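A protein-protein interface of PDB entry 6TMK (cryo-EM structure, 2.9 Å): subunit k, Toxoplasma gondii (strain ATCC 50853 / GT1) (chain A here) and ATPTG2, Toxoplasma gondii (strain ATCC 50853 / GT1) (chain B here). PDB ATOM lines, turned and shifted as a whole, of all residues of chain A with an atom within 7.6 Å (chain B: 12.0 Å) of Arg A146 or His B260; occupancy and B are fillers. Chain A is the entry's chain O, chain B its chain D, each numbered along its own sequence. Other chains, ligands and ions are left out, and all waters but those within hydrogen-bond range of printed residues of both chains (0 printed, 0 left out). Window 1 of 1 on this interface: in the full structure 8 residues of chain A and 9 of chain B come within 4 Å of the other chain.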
ATOM      1  N   CYS A 125     -19.715   7.189 -20.135  1.00  0.00           N
ATOM      2  CA  CYS A 125     -18.577   7.806 -19.466  1.00  0.00           C
ATOM      3  C   CYS A 125     -18.365   9.158 -20.122  1.00  0.00           C
ATOM      4  O   CYS A 125     -17.971   9.223 -21.288  1.00  0.00           O
ATOM      5  CB  CYS A 125     -17.330   6.941 -19.582  1.00  0.00           C
ATOM      6  SG  CYS A 125     -16.022   7.335 -18.419  1.00  0.00           S
ATOM      7  N   ARG A 126     -18.642  10.228 -19.383  1.00  0.00           N
ATOM      8  CA  ARG A 126     -18.492  11.580 -19.900  1.00  0.00           C
ATOM      9  C   ARG A 126     -19.453  11.834 -21.053  1.00  0.00           C
ATOM     10  O   ARG A 126     -19.142  12.573 -21.988  1.00  0.00           O
ATOM     11  CB  ARG A 126     -17.046  11.834 -20.323  1.00  0.00           C
ATOM     12  CG  ARG A 126     -16.675  13.272 -20.487  1.00  0.00           C
ATOM     13  CD  ARG A 126     -15.212  13.476 -20.188  1.00  0.00           C
ATOM     14  NE  ARG A 126     -14.998  13.667 -18.762  1.00  0.00           N
ATOM     15  CZ  ARG A 126     -14.970  14.854 -18.164  1.00  0.00           C
ATOM     16  NH1 ARG A 126     -15.143  15.965 -18.864  1.00  0.00           N
ATOM     17  NH2 ARG A 126     -14.776  14.933 -16.860  1.00  0.00           N
ATOM     18  N   VAL A 140     -12.760   3.141 -22.077  1.00  0.00           N
ATOM     19  CA  VAL A 140     -12.428   4.246 -21.189  1.00  0.00           C
ATOM     20  C   VAL A 140     -11.218   5.003 -21.715  1.00  0.00           C
ATOM     21  O   VAL A 140     -11.195   6.238 -21.718  1.00  0.00           O
ATOM     22  CB  VAL A 140     -12.197   3.721 -19.762  1.00  0.00           C
ATOM     23  CG1 VAL A 140     -11.543   4.773 -18.904  1.00  0.00           C
ATOM     24  CG2 VAL A 140     -13.498   3.277 -19.159  1.00  0.00           C
ATOM     25  N   ARG A 141     -10.205   4.276 -22.184  1.00  0.00           N
ATOM     26  CA  ARG A 141      -9.044   4.907 -22.795  1.00  0.00           C
ATOM     27  C   ARG A 141      -9.453   5.845 -23.921  1.00  0.00           C
ATOM     28  O   ARG A 141      -8.882   6.930 -24.079  1.00  0.00           O
ATOM     29  CB  ARG A 141      -8.105   3.825 -23.315  1.00  0.00           C
ATOM     30  CG  ARG A 141      -6.750   4.293 -23.739  1.00  0.00           C
ATOM     31  CD  ARG A 141      -6.027   3.174 -24.435  1.00  0.00           C
ATOM     32  NE  ARG A 141      -4.579   3.359 -24.469  1.00  0.00           N
ATOM     33  CZ  ARG A 141      -3.915   3.908 -25.478  1.00  0.00           C
ATOM     34  NH1 ARG A 141      -4.552   4.340 -26.554  1.00  0.00           N
ATOM     35  NH2 ARG A 141      -2.602   4.024 -25.409  1.00  0.00           N
ATOM     36  N   PHE A 143     -12.808   7.158 -24.629  1.00  0.00           N
ATOM     37  CA  PHE A 143     -13.811   8.175 -24.357  1.00  0.00           C
ATOM     38  C   PHE A 143     -13.444   9.032 -23.153  1.00  0.00           C
ATOM     39  O   PHE A 143     -13.500  10.264 -23.224  1.00  0.00           O
ATOM     40  CB  PHE A 143     -15.172   7.510 -24.171  1.00  0.00           C
ATOM     41  CG  PHE A 143     -15.668   6.811 -25.398  1.00  0.00           C
ATOM     42  CD1 PHE A 143     -15.987   5.475 -25.364  1.00  0.00           C
ATOM     43  CD2 PHE A 143     -15.810   7.493 -26.587  1.00  0.00           C
ATOM     44  CE1 PHE A 143     -16.440   4.834 -26.488  1.00  0.00           C
ATOM     45  CE2 PHE A 143     -16.261   6.855 -27.708  1.00  0.00           C
ATOM     46  CZ  PHE A 143     -16.571   5.524 -27.663  1.00  0.00           C
ATOM     47  N   CYS A 144     -13.085   8.407 -22.031  1.00  0.00           N
ATOM     48  CA  CYS A 144     -12.770   9.129 -20.798  1.00  0.00           C
ATOM     49  C   CYS A 144     -11.393   8.690 -20.309  1.00  0.00           C
ATOM     50  O   CYS A 144     -11.272   7.826 -19.440  1.00  0.00           O
ATOM     51  CB  CYS A 144     -13.837   8.893 -19.755  1.00  0.00           C
ATOM     52  SG  CYS A 144     -14.339   7.183 -19.540  1.00  0.00           S
ATOM     53  N   LYS A 145     -10.357   9.318 -20.847  1.00  0.00           N
ATOM     54  CA  LYS A 145      -8.992   9.021 -20.438  1.00  0.00           C
ATOM     55  C   LYS A 145      -8.747   9.594 -19.050  1.00  0.00           C
ATOM     56  O   LYS A 145      -8.845  10.808 -18.846  1.00  0.00           O
ATOM     57  CB  LYS A 145      -8.017   9.610 -21.450  1.00  0.00           C
ATOM     58  CG  LYS A 145      -6.580   9.169 -21.319  1.00  0.00           C
ATOM     59  CD  LYS A 145      -6.389   7.754 -21.784  1.00  0.00           C
ATOM     60  CE  LYS A 145      -4.973   7.517 -22.264  1.00  0.00           C
ATOM     61  NZ  LYS A 145      -3.969   7.697 -21.194  1.00  0.00           N
ATOM     62  N   ARG A 146      -8.425   8.721 -18.099  1.00  0.00           N
ATOM     63  CA  ARG A 146      -8.090   9.099 -16.731  1.00  0.00           C
ATOM     64  C   ARG A 146      -9.269   9.717 -15.990  1.00  0.00           C
ATOM     65  O   ARG A 146      -9.072  10.458 -15.024  1.00  0.00           O
ATOM     66  CB  ARG A 146      -6.895  10.053 -16.710  1.00  0.00           C
ATOM     67  CG  ARG A 146      -5.637   9.455 -17.294  1.00  0.00           C
ATOM     68  CD  ARG A 146      -4.554  10.491 -17.463  1.00  0.00           C
ATOM     69  NE  ARG A 146      -4.092  11.028 -16.191  1.00  0.00           N
ATOM     70  CZ  ARG A 146      -3.187  10.446 -15.416  1.00  0.00           C
ATOM     71  NH1 ARG A 146      -2.841  11.016 -14.275  1.00  0.00           N
ATOM     72  NH2 ARG A 146      -2.624   9.304 -15.775  1.00  0.00           N
ATOM     73  N   ASP A 147     -10.494   9.424 -16.422  1.00  0.00           N
ATOM     74  CA  ASP A 147     -11.709   9.757 -15.676  1.00  0.00           C
ATOM     75  C   ASP A 147     -12.676   8.588 -15.788  1.00  0.00           C
ATOM     76  O   ASP A 147     -13.675   8.648 -16.512  1.00  0.00           O
ATOM     77  CB  ASP A 147     -12.341  11.045 -16.202  1.00  0.00           C
ATOM     78  CG  ASP A 147     -13.480  11.524 -15.332  1.00  0.00           C
ATOM     79  OD1 ASP A 147     -13.231  11.796 -14.141  1.00  0.00           O
ATOM     80  OD2 ASP A 147     -14.622  11.621 -15.830  1.00  0.00           O
ATOM     81  N   PRO A 148     -12.410   7.503 -15.072  1.00  0.00           N
ATOM     82  CA  PRO A 148     -13.149   6.259 -15.320  1.00  0.00           C
ATOM     83  C   PRO A 148     -14.551   6.205 -14.736  1.00  0.00           C
ATOM     84  O   PRO A 148     -15.127   5.119 -14.629  1.00  0.00           O
ATOM     85  CB  PRO A 148     -12.254   5.194 -14.674  1.00  0.00           C
ATOM     86  CG  PRO A 148     -11.004   5.892 -14.262  1.00  0.00           C
ATOM     87  CD  PRO A 148     -11.345   7.307 -14.082  1.00  0.00           C
ATOM     88  N   ARG A 149     -15.114   7.344 -14.348  1.00  0.00           N
ATOM     89  CA  ARG A 149     -16.434   7.351 -13.737  1.00  0.00           C
ATOM     90  C   ARG A 149     -17.495   6.871 -14.720  1.00  0.00           C
ATOM     91  O   ARG A 149     -17.853   7.590 -15.656  1.00  0.00           O
ATOM     92  CB  ARG A 149     -16.750   8.750 -13.223  1.00  0.00           C
ATOM     93  CG  ARG A 149     -15.800   9.214 -12.149  1.00  0.00           C
ATOM     94  CD  ARG A 149     -16.049  10.640 -11.755  1.00  0.00           C
ATOM     95  NE  ARG A 149     -15.751  11.551 -12.851  1.00  0.00           N
ATOM     96  CZ  ARG A 149     -15.471  12.841 -12.701  1.00  0.00           C
ATOM     97  NH1 ARG A 149     -15.451  13.386 -11.497  1.00  0.00           N
ATOM     98  NH2 ARG A 149     -15.210  13.583 -13.764  1.00  0.00           N
ATOM     99  N   PHE B 255     -18.839  18.369 -17.698  1.00  0.00           N
ATOM    100  CA  PHE B 255     -18.646  17.343 -16.694  1.00  0.00           C
ATOM    101  C   PHE B 255     -17.495  17.757 -15.795  1.00  0.00           C
ATOM    102  O   PHE B 255     -16.568  18.437 -16.245  1.00  0.00           O
ATOM    103  CB  PHE B 255     -18.337  15.990 -17.346  1.00  0.00           C
ATOM    104  CG  PHE B 255     -19.383  15.534 -18.315  1.00  0.00           C
ATOM    105  CD1 PHE B 255     -20.529  14.907 -17.875  1.00  0.00           C
ATOM    106  CD2 PHE B 255     -19.228  15.752 -19.666  1.00  0.00           C
ATOM    107  CE1 PHE B 255     -21.488  14.498 -18.762  1.00  0.00           C
ATOM    108  CE2 PHE B 255     -20.187  15.346 -20.555  1.00  0.00           C
ATOM    109  CZ  PHE B 255     -21.320  14.719 -20.102  1.00  0.00           C
ATOM    110  N   PRO B 256     -17.525  17.372 -14.524  1.00  0.00           N
ATOM    111  CA  PRO B 256     -16.442  17.774 -13.623  1.00  0.00           C
ATOM    112  C   PRO B 256     -15.123  17.133 -14.009  1.00  0.00           C
ATOM    113  O   PRO B 256     -15.061  15.961 -14.386  1.00  0.00           O
ATOM    114  CB  PRO B 256     -16.931  17.292 -12.255  1.00  0.00           C
ATOM    115  CG  PRO B 256     -17.839  16.167 -12.568  1.00  0.00           C
ATOM    116  CD  PRO B 256     -18.526  16.547 -13.834  1.00  0.00           C
ATOM    117  N   ILE B 257     -14.063  17.924 -13.915  1.00  0.00           N
ATOM    118  CA  ILE B 257     -12.712  17.465 -14.217  1.00  0.00           C
ATOM    119  C   ILE B 257     -12.125  16.875 -12.943  1.00  0.00           C
ATOM    120  O   ILE B 257     -12.240  17.488 -11.872  1.00  0.00           O
ATOM    121  CB  ILE B 257     -11.857  18.606 -14.780  1.00  0.00           C
ATOM    122  CG1 ILE B 257     -12.363  18.964 -16.175  1.00  0.00           C
ATOM    123  CG2 ILE B 257     -10.394  18.202 -14.831  1.00  0.00           C
ATOM    124  CD1 ILE B 257     -12.013  20.341 -16.606  1.00  0.00           C
ATOM    125  N   PRO B 258     -11.519  15.693 -12.991  1.00  0.00           N
ATOM    126  CA  PRO B 258     -11.015  15.092 -11.757  1.00  0.00           C
ATOM    127  C   PRO B 258      -9.882  15.872 -11.099  1.00  0.00           C
ATOM    128  O   PRO B 258      -9.105  16.606 -11.732  1.00  0.00           O
ATOM    129  CB  PRO B 258     -10.550  13.702 -12.207  1.00  0.00           C
ATOM    130  CG  PRO B 258     -10.330  13.821 -13.657  1.00  0.00           C
ATOM    131  CD  PRO B 258     -11.353  14.789 -14.137  1.00  0.00           C
ATOM    132  N   ASP B 259      -9.786  15.662  -9.787  1.00  0.00           N
ATOM    133  CA  ASP B 259      -8.867  16.443  -8.982  1.00  0.00           C
ATOM    134  C   ASP B 259      -7.431  16.110  -9.339  1.00  0.00           C
ATOM    135  O   ASP B 259      -6.561  16.985  -9.295  1.00  0.00           O
ATOM    136  CB  ASP B 259      -9.131  16.188  -7.501  1.00  0.00           C
ATOM    137  CG  ASP B 259     -10.240  17.064  -6.944  1.00  0.00           C
ATOM    138  OD1 ASP B 259     -10.744  17.941  -7.677  1.00  0.00           O
ATOM    139  OD2 ASP B 259     -10.618  16.869  -5.769  1.00  0.00           O
ATOM    140  N   HIS B 260      -7.165  14.858  -9.707  1.00  0.00           N
ATOM    141  CA  HIS B 260      -5.814  14.465 -10.059  1.00  0.00           C
ATOM    142  C   HIS B 260      -5.427  14.955 -11.440  1.00  0.00           C
ATOM    143  O   HIS B 260      -4.300  14.706 -11.880  1.00  0.00           O
ATOM    144  CB  HIS B 260      -5.662  12.946  -9.982  1.00  0.00           C
ATOM    145  CG  HIS B 260      -6.505  12.196 -10.963  1.00  0.00           C
ATOM    146  ND1 HIS B 260      -7.781  11.765 -10.671  1.00  0.00           N
ATOM    147  CD2 HIS B 260      -6.249  11.786 -12.226  1.00  0.00           C
ATOM    148  CE1 HIS B 260      -8.276  11.127 -11.717  1.00  0.00           C
ATOM    149  NE2 HIS B 260      -7.368  11.128 -12.673  1.00  0.00           N
ATOM    150  N   GLU B 261      -6.332  15.655 -12.120  1.00  0.00           N
ATOM    151  CA  GLU B 261      -6.045  16.268 -13.399  1.00  0.00           C
ATOM    152  C   GLU B 261      -6.167  17.777 -13.322  1.00  0.00           C
ATOM    153  O   GLU B 261      -5.921  18.460 -14.323  1.00  0.00           O
ATOM    154  CB  GLU B 261      -6.981  15.715 -14.478  1.00  0.00           C
ATOM    155  CG  GLU B 261      -6.610  14.329 -14.968  1.00  0.00           C
ATOM    156  CD  GLU B 261      -5.431  14.340 -15.927  1.00  0.00           C
ATOM    157  OE1 GLU B 261      -5.466  15.117 -16.902  1.00  0.00           O
ATOM    158  OE2 GLU B 261      -4.467  13.578 -15.703  1.00  0.00           O
ATOM    159  N   GLN B 262      -6.537  18.318 -12.159  1.00  0.00           N
ATOM    160  CA  GLN B 262      -6.582  19.768 -12.062  1.00  0.00           C
ATOM    161  C   GLN B 262      -5.228  20.307 -11.597  1.00  0.00           C
ATOM    162  O   GLN B 262      -4.539  19.662 -10.803  1.00  0.00           O
ATOM    163  CB  GLN B 262      -7.673  20.212 -11.096  1.00  0.00           C
ATOM    164  CG  GLN B 262      -9.062  19.919 -11.589  1.00  0.00           C
ATOM    165  CD  GLN B 262     -10.076  20.884 -11.046  1.00  0.00           C
ATOM    166  OE1 GLN B 262     -10.622  20.689  -9.962  1.00  0.00           O
ATOM    167  NE2 GLN B 262     -10.316  21.954 -11.786  1.00  0.00           N
ATOM    168  N   PRO B 263      -4.801  21.479 -12.059  1.00  0.00           N
ATOM    169  CA  PRO B 263      -3.479  21.986 -11.694  1.00  0.00           C
ATOM    170  C   PRO B 263      -3.455  22.747 -10.375  1.00  0.00           C
ATOM    171  O   PRO B 263      -4.463  23.264  -9.897  1.00  0.00           O
ATOM    172  CB  PRO B 263      -3.145  22.914 -12.867  1.00  0.00           C
ATOM    173  CG  PRO B 263      -4.429  23.446 -13.267  1.00  0.00           C
ATOM    174  CD  PRO B 263      -5.450  22.361 -13.043  1.00  0.00           C
ATOM    175  N   TYR B 264      -2.258  22.819  -9.803  1.00  0.00           N
ATOM    176  CA  TYR B 264      -2.064  23.454  -8.511  1.00  0.00           C
ATOM    177  C   TYR B 264      -1.643  24.906  -8.655  1.00  0.00           C
ATOM    178  O   TYR B 264      -0.930  25.283  -9.588  1.00  0.00           O
ATOM    179  CB  TYR B 264      -0.983  22.738  -7.704  1.00  0.00           C
ATOM    180  CG  TYR B 264      -1.339  21.379  -7.169  1.00  0.00           C
ATOM    181  CD1 TYR B 264      -2.538  21.147  -6.528  1.00  0.00           C
ATOM    182  CD2 TYR B 264      -0.447  20.329  -7.286  1.00  0.00           C
ATOM    183  CE1 TYR B 264      -2.848  19.907  -6.038  1.00  0.00           C
ATOM    184  CE2 TYR B 264      -0.746  19.089  -6.799  1.00  0.00           C
ATOM    185  CZ  TYR B 264      -1.948  18.879  -6.173  1.00  0.00           C
ATOM    186  OH  TYR B 264      -2.251  17.635  -5.683  1.00  0.00           O
ATOM    187  N   ARG B 265      -2.089  25.716  -7.707  1.00  0.00           N
ATOM    188  CA  ARG B 265      -1.635  27.089  -7.593  1.00  0.00           C
ATOM    189  C   ARG B 265      -0.300  27.147  -6.863  1.00  0.00           C
ATOM    190  O   ARG B 265      -0.003  26.322  -5.995  1.00  0.00           O
ATOM    191  CB  ARG B 265      -2.671  27.926  -6.854  1.00  0.00           C
ATOM    192  CG  ARG B 265      -2.394  29.389  -6.830  1.00  0.00           C
ATOM    193  CD  ARG B 265      -3.519  30.121  -6.173  1.00  0.00           C
ATOM    194  NE  ARG B 265      -3.225  31.530  -5.975  1.00  0.00           N
ATOM    195  CZ  ARG B 265      -2.737  32.054  -4.860  1.00  0.00           C
ATOM    196  NH1 ARG B 265      -2.468  31.296  -3.812  1.00  0.00           N
ATOM    197  NH2 ARG B 265      -2.510  33.348  -4.798  1.00  0.00           N
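Among the printed residues, pairs that only touch across the chains: Arg A126 with Phe B255, Asp A147 with Pro B258 and Arg A146 with Pro B258.
The side-chain sulfur (SG) of Cys A125 forms a disulfide with the side-chain sulfur (SG) of Cys A144 (2.0 Å). The side-chain carboxylate (OD1) of Asp A147 lies within salt-bridge range of the guanidinium group (NH2) of Arg A149, at 2.7 Å. The side-chain carboxylate (OD2) of Asp A147 lies within salt-bridge range of the guanidinium group (NH2) of Arg A126, at 3.5 Å.
Of the printed residues of chain A, His B260 touches Arg A146. No residue of chain B comes within 4 Å of Cys A144. Lys A145 touches none of the printed residues of chain B. No residue of chain B comes within 4 Å of Pro A148. Printed residues of chain A within 4 Å of Pro B256: Arg A126 (2.7 Å) and Arg A149 (2.5 Å). Printed residues of chain A within 4 Å of Phe B255: Arg A126. Of the printed residues of chain B, Arg A126 touches Phe B255 and Pro B256. Of the printed residues of chain A, Glu B261 touches Arg A146. Printed residues of chain B within 4 Å of Arg A149: Pro B256 (2.5 Å). Asp B259 touches none of the printed residues of chain A. Tyr B264 touches none of the printed residues of chain A. The nearest printed residue of chain B that does not touch Arg A146 is Ile B257 (7.4 Å). The nearest residue of chain A that does not touch His B260 is Asp A147 (5.2 Å). The nearest printed residue of chain A that does not touch Phe B255 is Arg A149 (5.2 Å).
A ring nitrogen (NE2) of His B260 sits at hydrogen-bond distance from the backbone carbonyl oxygen (O) of Arg A146. The backbone carbonyl oxygen (O) of Pro B256 is in hydrogen-bond range of the guanidinium group (NH2) of Arg A126, at 2.7 Å. NE of Arg A146 lies within salt-bridge range of OE2 of Glu B261 (2.6 Å). O of Pro B256 sits at hydrogen-bond distance from NH2 of Arg A149.
Among the printed residues, Asp or Glu carboxylates within 4 Å of a Lys or Arg side-chain nitrogen of the other chain: Arg A146 with Glu B261 (2.6 Å).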
